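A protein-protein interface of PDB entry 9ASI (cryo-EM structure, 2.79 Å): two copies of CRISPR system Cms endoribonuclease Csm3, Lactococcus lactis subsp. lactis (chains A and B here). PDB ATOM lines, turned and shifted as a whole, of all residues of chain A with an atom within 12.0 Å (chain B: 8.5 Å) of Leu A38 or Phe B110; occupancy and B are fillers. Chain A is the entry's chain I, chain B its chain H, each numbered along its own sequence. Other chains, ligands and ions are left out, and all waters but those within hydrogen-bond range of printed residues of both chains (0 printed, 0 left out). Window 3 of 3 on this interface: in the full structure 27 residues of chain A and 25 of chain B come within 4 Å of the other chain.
Position printed for both chains: 104. Of the 12 pairs that touch across the chains among the printed residues, none has its exchanged pair printed and touching as well.
Of chain B, only Leu B107 (3.6 Å), Phe B110 (3.5 Å), Val B112 (3.6 Å), Ile B139 (3.9 Å), Ala B140 (3.7 Å) and Gly B141 (3.96 Å) come within 4 Å of Leu A38. No residue of chain A comes within 4 Å of Glu B106. Of chain A, only Leu A38 comes within 4 Å of Leu B107. No residue of chain A comes within 4 Å of Thr B109. Val B112 touches just these residues of chain A: Thr A37, Leu A38 and Arg A40. Ile B139 touches two residues of chain A. No residue of chain A comes within 4 Å of Ser B142. Printed residues of chain B within 4 Å of Arg A40: Phe B110 (2.9 Å), Asn B111 (3.4 Å) and Val B112 (3.3 Å). Of the printed residues of chain B, Thr A37 touches Val B112 (3.4 Å), Glu B116 (3.3 Å) and Ile B139 (3.7 Å). Printed residues of chain A within 4 Å of Glu B116: Thr A37 (3.3 Å). Leu A41 touches none of the printed residues of chain B. Val B10 touches none of the printed residues of chain A. The nearest residue of chain A that does not touch Phe B110 is Thr A37 (5.8 Å).
The backbone carbonyl oxygen (O) of Asn B111 lies within hydrogen-bond range of the guanidinium group (NH2) of Arg A40 (3.4 Å). The backbone carbonyl oxygen (O) of Phe B110 is in hydrogen-bond range of the guanidinium group (NH1) of Arg A40 (2.9 Å).
N of Gly B141 sits at hydrogen-bond distance from O of Leu B11, 3.0 Å away. O of Leu B107 sits close to N of Val B112, at 3.4 Å. The backbone carbonyl oxygen (O) of Ile B139 lies within hydrogen-bond range of the side-chain hydroxyl (OG) of Ser B142 (2.5 Å). NE of Arg A35 is in hydrogen-bond range of O of Arg A40, at 3.4 Å. ND2 of Asn B103 is in hydrogen-bond range of O of Gly B141 (3.0 Å). The backbone NH of Ile B139 lies within hydrogen-bond range of the backbone carbonyl oxygen of Ser B114 (3.1 Å).
Among the printed residues, pairs that only touch across the chains: Thr A37 with Val B112, Thr A37 with Glu B116, Thr A37 with Ile B139, Leu A38 with Leu B107, Leu A38 with Phe B110, Leu A38 with Val B112, Leu A38 with Ile B139, Leu A38 with Ala B140, Leu A38 with Gly B141 and Arg A40 with Val B112.
Hydrophobic or aromatic side chains of chain B within 4 Å of the printed part of chain A: Leu B107, Phe B110, Val B112 and Ile B139. Printed residues of chain A that touch a printed residue of chain B: Thr A37, Leu A38 and Arg A40. Among the printed residues, 12 pairs touch across the chains. Among the printed residues, no Asp or Glu carboxylate lies within 4 Å of a Lys or Arg side-chain nitrogen of the other chain.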
ATOM      1  N   GLY A  19     -17.340   0.125 -11.361  1.00  0.00           N
ATOM      2  CA  GLY A  19     -16.980   1.456 -11.802  1.00  0.00           C
ATOM      3  C   GLY A  19     -17.367   2.537 -10.815  1.00  0.00           C
ATOM      4  O   GLY A  19     -17.468   3.712 -11.179  1.00  0.00           O
ATOM      5  N   ASP A  22     -16.416   5.485  -4.854  1.00  0.00           N
ATOM      6  CA  ASP A  22     -16.776   5.886  -3.505  1.00  0.00           C
ATOM      7  C   ASP A  22     -16.093   4.979  -2.489  1.00  0.00           C
ATOM      8  O   ASP A  22     -15.659   3.867  -2.805  1.00  0.00           O
ATOM      9  CB  ASP A  22     -18.297   5.858  -3.300  1.00  0.00           C
ATOM     10  CG  ASP A  22     -18.927   4.562  -3.766  1.00  0.00           C
ATOM     11  OD1 ASP A  22     -18.584   3.497  -3.212  1.00  0.00           O
ATOM     12  OD2 ASP A  22     -19.770   4.608  -4.684  1.00  0.00           O
ATOM     13  N   VAL A  33     -22.086  -1.266  -7.617  1.00  0.00           N
ATOM     14  CA  VAL A  33     -22.388  -1.255  -9.034  1.00  0.00           C
ATOM     15  C   VAL A  33     -22.141   0.140  -9.594  1.00  0.00           C
ATOM     16  O   VAL A  33     -21.974   1.111  -8.860  1.00  0.00           O
ATOM     17  CB  VAL A  33     -23.841  -1.710  -9.315  1.00  0.00           C
ATOM     18  CG1 VAL A  33     -24.037  -3.141  -8.887  1.00  0.00           C
ATOM     19  CG2 VAL A  33     -24.831  -0.799  -8.610  1.00  0.00           C
ATOM     20  N   VAL A  34     -22.111   0.242 -10.916  1.00  0.00           N
ATOM     21  CA  VAL A  34     -22.019   1.537 -11.577  1.00  0.00           C
ATOM     22  C   VAL A  34     -23.409   2.161 -11.617  1.00  0.00           C
ATOM     23  O   VAL A  34     -24.388   1.513 -12.006  1.00  0.00           O
ATOM     24  CB  VAL A  34     -21.414   1.394 -12.984  1.00  0.00           C
ATOM     25  CG1 VAL A  34     -22.246   0.472 -13.842  1.00  0.00           C
ATOM     26  CG2 VAL A  34     -21.271   2.747 -13.645  1.00  0.00           C
ATOM     27  N   ARG A  35     -23.509   3.410 -11.172  1.00  0.00           N
ATOM     28  CA  ARG A  35     -24.777   4.115 -11.136  1.00  0.00           C
ATOM     29  C   ARG A  35     -24.603   5.511 -11.710  1.00  0.00           C
ATOM     30  O   ARG A  35     -23.490   6.029 -11.813  1.00  0.00           O
ATOM     31  CB  ARG A  35     -25.346   4.215  -9.716  1.00  0.00           C
ATOM     32  CG  ARG A  35     -25.021   3.051  -8.810  1.00  0.00           C
ATOM     33  CD  ARG A  35     -25.284   3.410  -7.362  1.00  0.00           C
ATOM     34  NE  ARG A  35     -26.691   3.242  -7.023  1.00  0.00           N
ATOM     35  CZ  ARG A  35     -27.188   2.190  -6.390  1.00  0.00           C
ATOM     36  NH1 ARG A  35     -26.413   1.201  -5.980  1.00  0.00           N
ATOM     37  NH2 ARG A  35     -28.496   2.127  -6.165  1.00  0.00           N
ATOM     38  N   ASP A  36     -25.727   6.109 -12.096  1.00  0.00           N
ATOM     39  CA  ASP A  36     -25.727   7.499 -12.523  1.00  0.00           C
ATOM     40  C   ASP A  36     -25.384   8.402 -11.348  1.00  0.00           C
ATOM     41  O   ASP A  36     -25.792   8.153 -10.212  1.00  0.00           O
ATOM     42  CB  ASP A  36     -27.088   7.878 -13.100  1.00  0.00           C
ATOM     43  CG  ASP A  36     -27.084   9.242 -13.762  1.00  0.00           C
ATOM     44  OD1 ASP A  36     -25.991   9.808 -13.968  1.00  0.00           O
ATOM     45  OD2 ASP A  36     -28.178   9.755 -14.072  1.00  0.00           O
ATOM     46  N   THR A  37     -24.616   9.457 -11.624  1.00  0.00           N
ATOM     47  CA  THR A  37     -24.166  10.336 -10.551  1.00  0.00           C
ATOM     48  C   THR A  37     -25.305  11.195 -10.017  1.00  0.00           C
ATOM     49  O   THR A  37     -25.469  11.335  -8.800  1.00  0.00           O
ATOM     50  CB  THR A  37     -23.017  11.211 -11.048  1.00  0.00           C
ATOM     51  OG1 THR A  37     -21.909  10.378 -11.409  1.00  0.00           O
ATOM     52  CG2 THR A  37     -22.576  12.182  -9.971  1.00  0.00           C
ATOM     53  N   LEU A  38     -26.111  11.764 -10.911  1.00  0.00           N
ATOM     54  CA  LEU A  38     -27.153  12.699 -10.504  1.00  0.00           C
ATOM     55  C   LEU A  38     -28.357  11.979  -9.910  1.00  0.00           C
ATOM     56  O   LEU A  38     -28.796  12.301  -8.801  1.00  0.00           O
ATOM     57  CB  LEU A  38     -27.580  13.549 -11.700  1.00  0.00           C
ATOM     58  CG  LEU A  38     -28.416  14.792 -11.414  1.00  0.00           C
ATOM     59  CD1 LEU A  38     -27.540  15.872 -10.831  1.00  0.00           C
ATOM     60  CD2 LEU A  38     -29.097  15.278 -12.675  1.00  0.00           C
ATOM     61  N   THR A  39     -28.908  11.007 -10.635  1.00  0.00           N
ATOM     62  CA  THR A  39     -30.126  10.329 -10.217  1.00  0.00           C
ATOM     63  C   THR A  39     -29.876   9.122  -9.323  1.00  0.00           C
ATOM     64  O   THR A  39     -30.839   8.569  -8.780  1.00  0.00           O
ATOM     65  CB  THR A  39     -30.932   9.884 -11.443  1.00  0.00           C
ATOM     66  OG1 THR A  39     -30.048   9.342 -12.430  1.00  0.00           O
ATOM     67  CG2 THR A  39     -31.688  11.059 -12.037  1.00  0.00           C
ATOM     68  N   ARG A  40     -28.620   8.703  -9.160  1.00  0.00           N
ATOM     69  CA  ARG A  40     -28.259   7.561  -8.317  1.00  0.00           C
ATOM     70  C   ARG A  40     -28.946   6.277  -8.774  1.00  0.00           C
ATOM     71  O   ARG A  40     -29.216   5.385  -7.968  1.00  0.00           O
ATOM     72  CB  ARG A  40     -28.568   7.833  -6.844  1.00  0.00           C
ATOM     73  CG  ARG A  40     -27.396   8.383  -6.061  1.00  0.00           C
ATOM     74  CD  ARG A  40     -27.487   9.890  -5.936  1.00  0.00           C
ATOM     75  NE  ARG A  40     -26.319  10.451  -5.270  1.00  0.00           N
ATOM     76  CZ  ARG A  40     -26.122  11.746  -5.070  1.00  0.00           C
ATOM     77  NH1 ARG A  40     -27.002  12.648  -5.472  1.00  0.00           N
ATOM     78  NH2 ARG A  40     -25.015  12.146  -4.454  1.00  0.00           N
ATOM     79  N   LEU A  41     -29.222   6.172 -10.047  1.00  0.00           N
ATOM     80  CA  LEU A  41     -29.869   4.982 -10.563  1.00  0.00           C
ATOM     81  C   LEU A  41     -28.841   4.042 -11.174  1.00  0.00           C
ATOM     82  O   LEU A  41     -27.853   4.495 -11.756  1.00  0.00           O
ATOM     83  CB  LEU A  41     -30.912   5.347 -11.622  1.00  0.00           C
ATOM     84  CG  LEU A  41     -32.265   5.815 -11.093  1.00  0.00           C
ATOM     85  CD1 LEU A  41     -33.051   6.498 -12.190  1.00  0.00           C
ATOM     86  CD2 LEU A  41     -33.043   4.649 -10.519  1.00  0.00           C
ATOM     87  N   PRO A  42     -29.051   2.730 -11.060  1.00  0.00           N
ATOM     88  CA  PRO A  42     -28.122   1.782 -11.678  1.00  0.00           C
ATOM     89  C   PRO A  42     -28.042   1.992 -13.180  1.00  0.00           C
ATOM     90  O   PRO A  42     -29.022   2.342 -13.838  1.00  0.00           O
ATOM     91  CB  PRO A  42     -28.724   0.418 -11.329  1.00  0.00           C
ATOM     92  CG  PRO A  42     -29.499   0.672 -10.090  1.00  0.00           C
ATOM     93  CD  PRO A  42     -30.082   2.041 -10.266  1.00  0.00           C
ATOM     94  N   LEU A  43     -26.850   1.775 -13.715  1.00  0.00           N
ATOM     95  CA  LEU A  43     -26.516   2.150 -15.078  1.00  0.00           C
ATOM     96  C   LEU A  43     -25.944   0.945 -15.805  1.00  0.00           C
ATOM     97  O   LEU A  43     -25.167   0.177 -15.231  1.00  0.00           O
ATOM     98  CB  LEU A  43     -25.493   3.294 -15.072  1.00  0.00           C
ATOM     99  CG  LEU A  43     -25.009   3.933 -16.371  1.00  0.00           C
ATOM    100  CD1 LEU A  43     -26.154   4.600 -17.104  1.00  0.00           C
ATOM    101  CD2 LEU A  43     -23.896   4.917 -16.088  1.00  0.00           C
ATOM    102  N   ASP A  98     -25.334   5.051 -22.834  1.00  0.00           N
ATOM    103  CA  ASP A  98     -25.374   4.581 -21.457  1.00  0.00           C
ATOM    104  C   ASP A  98     -26.817   4.397 -21.013  1.00  0.00           C
ATOM    105  O   ASP A  98     -27.597   5.353 -20.981  1.00  0.00           O
ATOM    106  CB  ASP A  98     -24.649   5.566 -20.546  1.00  0.00           C
ATOM    107  CG  ASP A  98     -23.152   5.521 -20.726  1.00  0.00           C
ATOM    108  OD1 ASP A  98     -22.664   4.591 -21.395  1.00  0.00           O
ATOM    109  OD2 ASP A  98     -22.459   6.417 -20.201  1.00  0.00           O
ATOM    110  N   LYS A 100     -29.862   3.700 -18.608  1.00  0.00           N
ATOM    111  CA  LYS A 100     -30.203   3.959 -17.217  1.00  0.00           C
ATOM    112  C   LYS A 100     -31.395   3.109 -16.797  1.00  0.00           C
ATOM    113  O   LYS A 100     -32.203   2.689 -17.628  1.00  0.00           O
ATOM    114  CB  LYS A 100     -30.513   5.440 -17.001  1.00  0.00           C
ATOM    115  CG  LYS A 100     -30.429   5.889 -15.555  1.00  0.00           C
ATOM    116  CD  LYS A 100     -30.309   7.395 -15.453  1.00  0.00           C
ATOM    117  CE  LYS A 100     -31.584   8.081 -15.910  1.00  0.00           C
ATOM    118  NZ  LYS A 100     -31.534   9.553 -15.697  1.00  0.00           N
ATOM    119  N   LEU A 101     -31.491   2.852 -15.495  1.00  0.00           N
ATOM    120  CA  LEU A 101     -32.594   2.061 -14.970  1.00  0.00           C
ATOM    121  C   LEU A 101     -33.913   2.800 -15.155  1.00  0.00           C
ATOM    122  O   LEU A 101     -33.994   4.018 -14.977  1.00  0.00           O
ATOM    123  CB  LEU A 101     -32.371   1.747 -13.492  1.00  0.00           C
ATOM    124  CG  LEU A 101     -33.358   0.740 -12.900  1.00  0.00           C
ATOM    125  CD1 LEU A 101     -32.845  -0.663 -13.097  1.00  0.00           C
ATOM    126  CD2 LEU A 101     -33.614   1.021 -11.433  1.00  0.00           C
ATOM    127  N   LEU A 104     -38.112   1.892 -11.836  1.00  0.00           N
ATOM    128  CA  LEU A 104     -38.008   2.112 -10.399  1.00  0.00           C
ATOM    129  C   LEU A 104     -39.381   2.156  -9.739  1.00  0.00           C
ATOM    130  O   LEU A 104     -39.502   1.859  -8.546  1.00  0.00           O
ATOM    131  CB  LEU A 104     -37.237   3.399 -10.113  1.00  0.00           C
ATOM    132  CG  LEU A 104     -36.804   3.606  -8.659  1.00  0.00           C
ATOM    133  CD1 LEU A 104     -35.611   2.725  -8.326  1.00  0.00           C
ATOM    134  CD2 LEU A 104     -36.490   5.067  -8.392  1.00  0.00           C
ATOM    135  N   VAL B  10     -28.405  20.166 -22.872  1.00  0.00           N
ATOM    136  CA  VAL B  10     -28.574  19.292 -21.719  1.00  0.00           C
ATOM    137  C   VAL B  10     -27.928  17.956 -22.042  1.00  0.00           C
ATOM    138  O   VAL B  10     -28.197  17.370 -23.096  1.00  0.00           O
ATOM    139  CB  VAL B  10     -30.058  19.110 -21.361  1.00  0.00           C
ATOM    140  CG1 VAL B  10     -30.197  18.365 -20.048  1.00  0.00           C
ATOM    141  CG2 VAL B  10     -30.751  20.453 -21.298  1.00  0.00           C
ATOM    142  N   LEU B  11     -27.067  17.485 -21.149  1.00  0.00           N
ATOM    143  CA  LEU B  11     -26.434  16.188 -21.337  1.00  0.00           C
ATOM    144  C   LEU B  11     -27.430  15.080 -21.024  1.00  0.00           C
ATOM    145  O   LEU B  11     -28.084  15.098 -19.978  1.00  0.00           O
ATOM    146  CB  LEU B  11     -25.200  16.058 -20.449  1.00  0.00           C
ATOM    147  CG  LEU B  11     -24.122  17.126 -20.608  1.00  0.00           C
ATOM    148  CD1 LEU B  11     -22.846  16.666 -19.952  1.00  0.00           C
ATOM    149  CD2 LEU B  11     -23.885  17.432 -22.070  1.00  0.00           C
ATOM    150  N   ASN B 103     -25.908  25.204 -14.966  1.00  0.00           N
ATOM    151  CA  ASN B 103     -26.689  24.747 -13.816  1.00  0.00           C
ATOM    152  C   ASN B 103     -25.820  24.071 -12.758  1.00  0.00           C
ATOM    153  O   ASN B 103     -26.131  22.987 -12.279  1.00  0.00           O
ATOM    154  CB  ASN B 103     -27.804  23.820 -14.287  1.00  0.00           C
ATOM    155  CG  ASN B 103     -27.286  22.502 -14.816  1.00  0.00           C
ATOM    156  OD1 ASN B 103     -26.121  22.382 -15.183  1.00  0.00           O
ATOM    157  ND2 ASN B 103     -28.149  21.497 -14.844  1.00  0.00           N
ATOM    158  N   LEU B 104     -24.735  24.727 -12.347  1.00  0.00           N
ATOM    159  CA  LEU B 104     -23.923  24.153 -11.281  1.00  0.00           C
ATOM    160  C   LEU B 104     -24.616  24.265  -9.929  1.00  0.00           C
ATOM    161  O   LEU B 104     -24.447  23.388  -9.079  1.00  0.00           O
ATOM    162  CB  LEU B 104     -22.547  24.815 -11.230  1.00  0.00           C
ATOM    163  CG  LEU B 104     -21.588  24.167 -10.229  1.00  0.00           C
ATOM    164  CD1 LEU B 104     -21.262  22.744 -10.640  1.00  0.00           C
ATOM    165  CD2 LEU B 104     -20.324  24.986 -10.060  1.00  0.00           C
ATOM    166  N   ALA B 105     -25.392  25.327  -9.708  1.00  0.00           N
ATOM    167  CA  ALA B 105     -26.167  25.422  -8.475  1.00  0.00           C
ATOM    168  C   ALA B 105     -27.223  24.325  -8.405  1.00  0.00           C
ATOM    169  O   ALA B 105     -27.448  23.735  -7.340  1.00  0.00           O
ATOM    170  CB  ALA B 105     -26.814  26.801  -8.365  1.00  0.00           C
ATOM    171  N   GLU B 106     -27.875  24.037  -9.532  1.00  0.00           N
ATOM    172  CA  GLU B 106     -28.838  22.942  -9.578  1.00  0.00           C
ATOM    173  C   GLU B 106     -28.166  21.608  -9.277  1.00  0.00           C
ATOM    174  O   GLU B 106     -28.731  20.765  -8.570  1.00  0.00           O
ATOM    175  CB  GLU B 106     -29.522  22.915 -10.944  1.00  0.00           C
ATOM    176  CG  GLU B 106     -30.248  21.621 -11.268  1.00  0.00           C
ATOM    177  CD  GLU B 106     -31.163  21.754 -12.472  1.00  0.00           C
ATOM    178  OE1 GLU B 106     -30.846  22.553 -13.379  1.00  0.00           O
ATOM    179  OE2 GLU B 106     -32.201  21.061 -12.513  1.00  0.00           O
ATOM    180  N   LEU B 107     -26.960  21.396  -9.808  1.00  0.00           N
ATOM    181  CA  LEU B 107     -26.219  20.176  -9.504  1.00  0.00           C
ATOM    182  C   LEU B 107     -25.836  20.110  -8.031  1.00  0.00           C
ATOM    183  O   LEU B 107     -25.910  19.042  -7.414  1.00  0.00           O
ATOM    184  CB  LEU B 107     -24.974  20.080 -10.386  1.00  0.00           C
ATOM    185  CG  LEU B 107     -25.189  19.979 -11.898  1.00  0.00           C
ATOM    186  CD1 LEU B 107     -23.897  19.610 -12.603  1.00  0.00           C
ATOM    187  CD2 LEU B 107     -26.289  18.991 -12.231  1.00  0.00           C
ATOM    188  N   GLU B 108     -25.419  21.237  -7.450  1.00  0.00           N
ATOM    189  CA  GLU B 108     -25.016  21.241  -6.048  1.00  0.00           C
ATOM    190  C   GLU B 108     -26.207  21.039  -5.122  1.00  0.00           C
ATOM    191  O   GLU B 108     -26.037  20.577  -3.989  1.00  0.00           O
ATOM    192  CB  GLU B 108     -24.293  22.543  -5.702  1.00  0.00           C
ATOM    193  CG  GLU B 108     -22.953  22.734  -6.402  1.00  0.00           C
ATOM    194  CD  GLU B 108     -21.913  21.698  -6.006  1.00  0.00           C
ATOM    195  OE1 GLU B 108     -22.053  21.078  -4.930  1.00  0.00           O
ATOM    196  OE2 GLU B 108     -20.947  21.507  -6.774  1.00  0.00           O
ATOM    197  N   THR B 109     -27.412  21.384  -5.578  1.00  0.00           N
ATOM    198  CA  THR B 109     -28.606  21.057  -4.805  1.00  0.00           C
ATOM    199  C   THR B 109     -28.739  19.549  -4.624  1.00  0.00           C
ATOM    200  O   THR B 109     -29.101  19.075  -3.541  1.00  0.00           O
ATOM    201  CB  THR B 109     -29.846  21.633  -5.487  1.00  0.00           C
ATOM    202  OG1 THR B 109     -29.759  23.063  -5.508  1.00  0.00           O
ATOM    203  CG2 THR B 109     -31.106  21.229  -4.743  1.00  0.00           C
ATOM    204  N   PHE B 110     -28.434  18.781  -5.669  1.00  0.00           N
ATOM    205  CA  PHE B 110     -28.456  17.325  -5.622  1.00  0.00           C
ATOM    206  C   PHE B 110     -27.199  16.731  -4.996  1.00  0.00           C
ATOM    207  O   PHE B 110     -26.996  15.516  -5.094  1.00  0.00           O
ATOM    208  CB  PHE B 110     -28.649  16.759  -7.030  1.00  0.00           C
ATOM    209  CG  PHE B 110     -30.039  16.930  -7.561  1.00  0.00           C
ATOM    210  CD1 PHE B 110     -31.092  17.206  -6.705  1.00  0.00           C
ATOM    211  CD2 PHE B 110     -30.298  16.822  -8.916  1.00  0.00           C
ATOM    212  CE1 PHE B 110     -32.374  17.367  -7.189  1.00  0.00           C
ATOM    213  CE2 PHE B 110     -31.579  16.981  -9.407  1.00  0.00           C
ATOM    214  CZ  PHE B 110     -32.617  17.253  -8.543  1.00  0.00           C
ATOM    215  N   ASN B 111     -26.361  17.558  -4.369  1.00  0.00           N
ATOM    216  CA  ASN B 111     -25.167  17.103  -3.654  1.00  0.00           C
ATOM    217  C   ASN B 111     -24.242  16.286  -4.551  1.00  0.00           C
ATOM    218  O   ASN B 111     -23.704  15.255  -4.142  1.00  0.00           O
ATOM    219  CB  ASN B 111     -25.545  16.312  -2.401  1.00  0.00           C
ATOM    220  CG  ASN B 111     -25.625  17.183  -1.164  1.00  0.00           C
ATOM    221  OD1 ASN B 111     -24.627  17.756  -0.728  1.00  0.00           O
ATOM    222  ND2 ASN B 111     -26.818  17.291  -0.594  1.00  0.00           N
ATOM    223  N   VAL B 112     -24.054  16.745  -5.786  1.00  0.00           N
ATOM    224  CA  VAL B 112     -23.104  16.142  -6.712  1.00  0.00           C
ATOM    225  C   VAL B 112     -22.267  17.238  -7.352  1.00  0.00           C
ATOM    226  O   VAL B 112     -22.697  18.390  -7.469  1.00  0.00           O
ATOM    227  CB  VAL B 112     -23.794  15.296  -7.805  1.00  0.00           C
ATOM    228  CG1 VAL B 112     -24.552  14.140  -7.192  1.00  0.00           C
ATOM    229  CG2 VAL B 112     -24.720  16.160  -8.634  1.00  0.00           C
ATOM    230  N   SER B 113     -21.057  16.871  -7.757  1.00  0.00           N
ATOM    231  CA  SER B 113     -20.232  17.749  -8.565  1.00  0.00           C
ATOM    232  C   SER B 113     -20.623  17.617 -10.035  1.00  0.00           C
ATOM    233  O   SER B 113     -21.427  16.764 -10.418  1.00  0.00           O
ATOM    234  CB  SER B 113     -18.752  17.431  -8.362  1.00  0.00           C
ATOM    235  OG  SER B 113     -18.455  16.100  -8.743  1.00  0.00           O
ATOM    236  N   SER B 114     -20.047  18.480 -10.866  1.00  0.00           N
ATOM    237  CA  SER B 114     -20.416  18.516 -12.273  1.00  0.00           C
ATOM    238  C   SER B 114     -19.744  17.430 -13.099  1.00  0.00           C
ATOM    239  O   SER B 114     -20.154  17.204 -14.241  1.00  0.00           O
ATOM    240  CB  SER B 114     -20.083  19.885 -12.866  1.00  0.00           C
ATOM    241  OG  SER B 114     -18.748  20.252 -12.572  1.00  0.00           O
ATOM    242  N   GLU B 116     -18.026  13.329 -13.236  1.00  0.00           N
ATOM    243  CA  GLU B 116     -17.919  11.989 -12.687  1.00  0.00           C
ATOM    244  C   GLU B 116     -16.644  11.335 -13.195  1.00  0.00           C
ATOM    245  O   GLU B 116     -15.932  11.874 -14.044  1.00  0.00           O
ATOM    246  CB  GLU B 116     -19.130  11.140 -13.080  1.00  0.00           C
ATOM    247  CG  GLU B 116     -19.040  10.607 -14.502  1.00  0.00           C
ATOM    248  CD  GLU B 116     -20.231   9.770 -14.900  1.00  0.00           C
ATOM    249  OE1 GLU B 116     -20.301   8.598 -14.477  1.00  0.00           O
ATOM    250  OE2 GLU B 116     -21.092  10.279 -15.646  1.00  0.00           O
ATOM    251  N   ILE B 139     -21.327  14.876 -15.907  1.00  0.00           N
ATOM    252  CA  ILE B 139     -22.450  14.006 -15.593  1.00  0.00           C
ATOM    253  C   ILE B 139     -23.668  14.386 -16.426  1.00  0.00           C
ATOM    254  O   ILE B 139     -23.844  15.542 -16.830  1.00  0.00           O
ATOM    255  CB  ILE B 139     -22.767  14.065 -14.087  1.00  0.00           C
ATOM    256  CG1 ILE B 139     -23.340  15.430 -13.710  1.00  0.00           C
ATOM    257  CG2 ILE B 139     -21.524  13.789 -13.278  1.00  0.00           C
ATOM    258  CD1 ILE B 139     -23.916  15.483 -12.321  1.00  0.00           C
ATOM    259  N   ALA B 140     -24.515  13.395 -16.690  1.00  0.00           N
ATOM    260  CA  ALA B 140     -25.786  13.659 -17.341  1.00  0.00           C
ATOM    261  C   ALA B 140     -26.647  14.548 -16.455  1.00  0.00           C
ATOM    262  O   ALA B 140     -26.541  14.528 -15.227  1.00  0.00           O
ATOM    263  CB  ALA B 140     -26.515  12.351 -17.643  1.00  0.00           C
ATOM    264  N   GLY B 141     -27.500  15.343 -17.091  1.00  0.00           N
ATOM    265  CA  GLY B 141     -28.274  16.342 -16.395  1.00  0.00           C
ATOM    266  C   GLY B 141     -27.610  17.694 -16.304  1.00  0.00           C
ATOM    267  O   GLY B 141     -28.258  18.657 -15.880  1.00  0.00           O
ATOM    268  N   SER B 142     -26.338  17.794 -16.683  1.00  0.00           N
ATOM    269  CA  SER B 142     -25.673  19.083 -16.769  1.00  0.00           C
ATOM    270  C   SER B 142     -26.263  19.890 -17.915  1.00  0.00           C
ATOM    271  O   SER B 142     -26.600  19.343 -18.968  1.00  0.00           O
ATOM    272  CB  SER B 142     -24.174  18.892 -16.981  1.00  0.00           C
ATOM    273  OG  SER B 142     -23.652  17.930 -16.089  1.00  0.00           O
ATOM    274  N   LYS B 143     -26.389  21.197 -17.712  1.00  0.00           N
ATOM    275  CA  LYS B 143     -26.958  22.090 -18.710  1.00  0.00           C
ATOM    276  C   LYS B 143     -25.929  23.139 -19.098  1.00  0.00           C
ATOM    277  O   LYS B 143     -25.277  23.726 -18.230  1.00  0.00           O
ATOM    278  CB  LYS B 143     -28.235  22.752 -18.193  1.00  0.00           C
ATOM    279  CG  LYS B 143     -29.401  21.791 -18.077  1.00  0.00           C
ATOM    280  CD  LYS B 143     -30.626  22.453 -17.492  1.00  0.00           C
ATOM    281  CE  LYS B 143     -31.756  21.454 -17.330  1.00  0.00           C
ATOM    282  NZ  LYS B 143     -32.977  22.078 -16.755  1.00  0.00           N
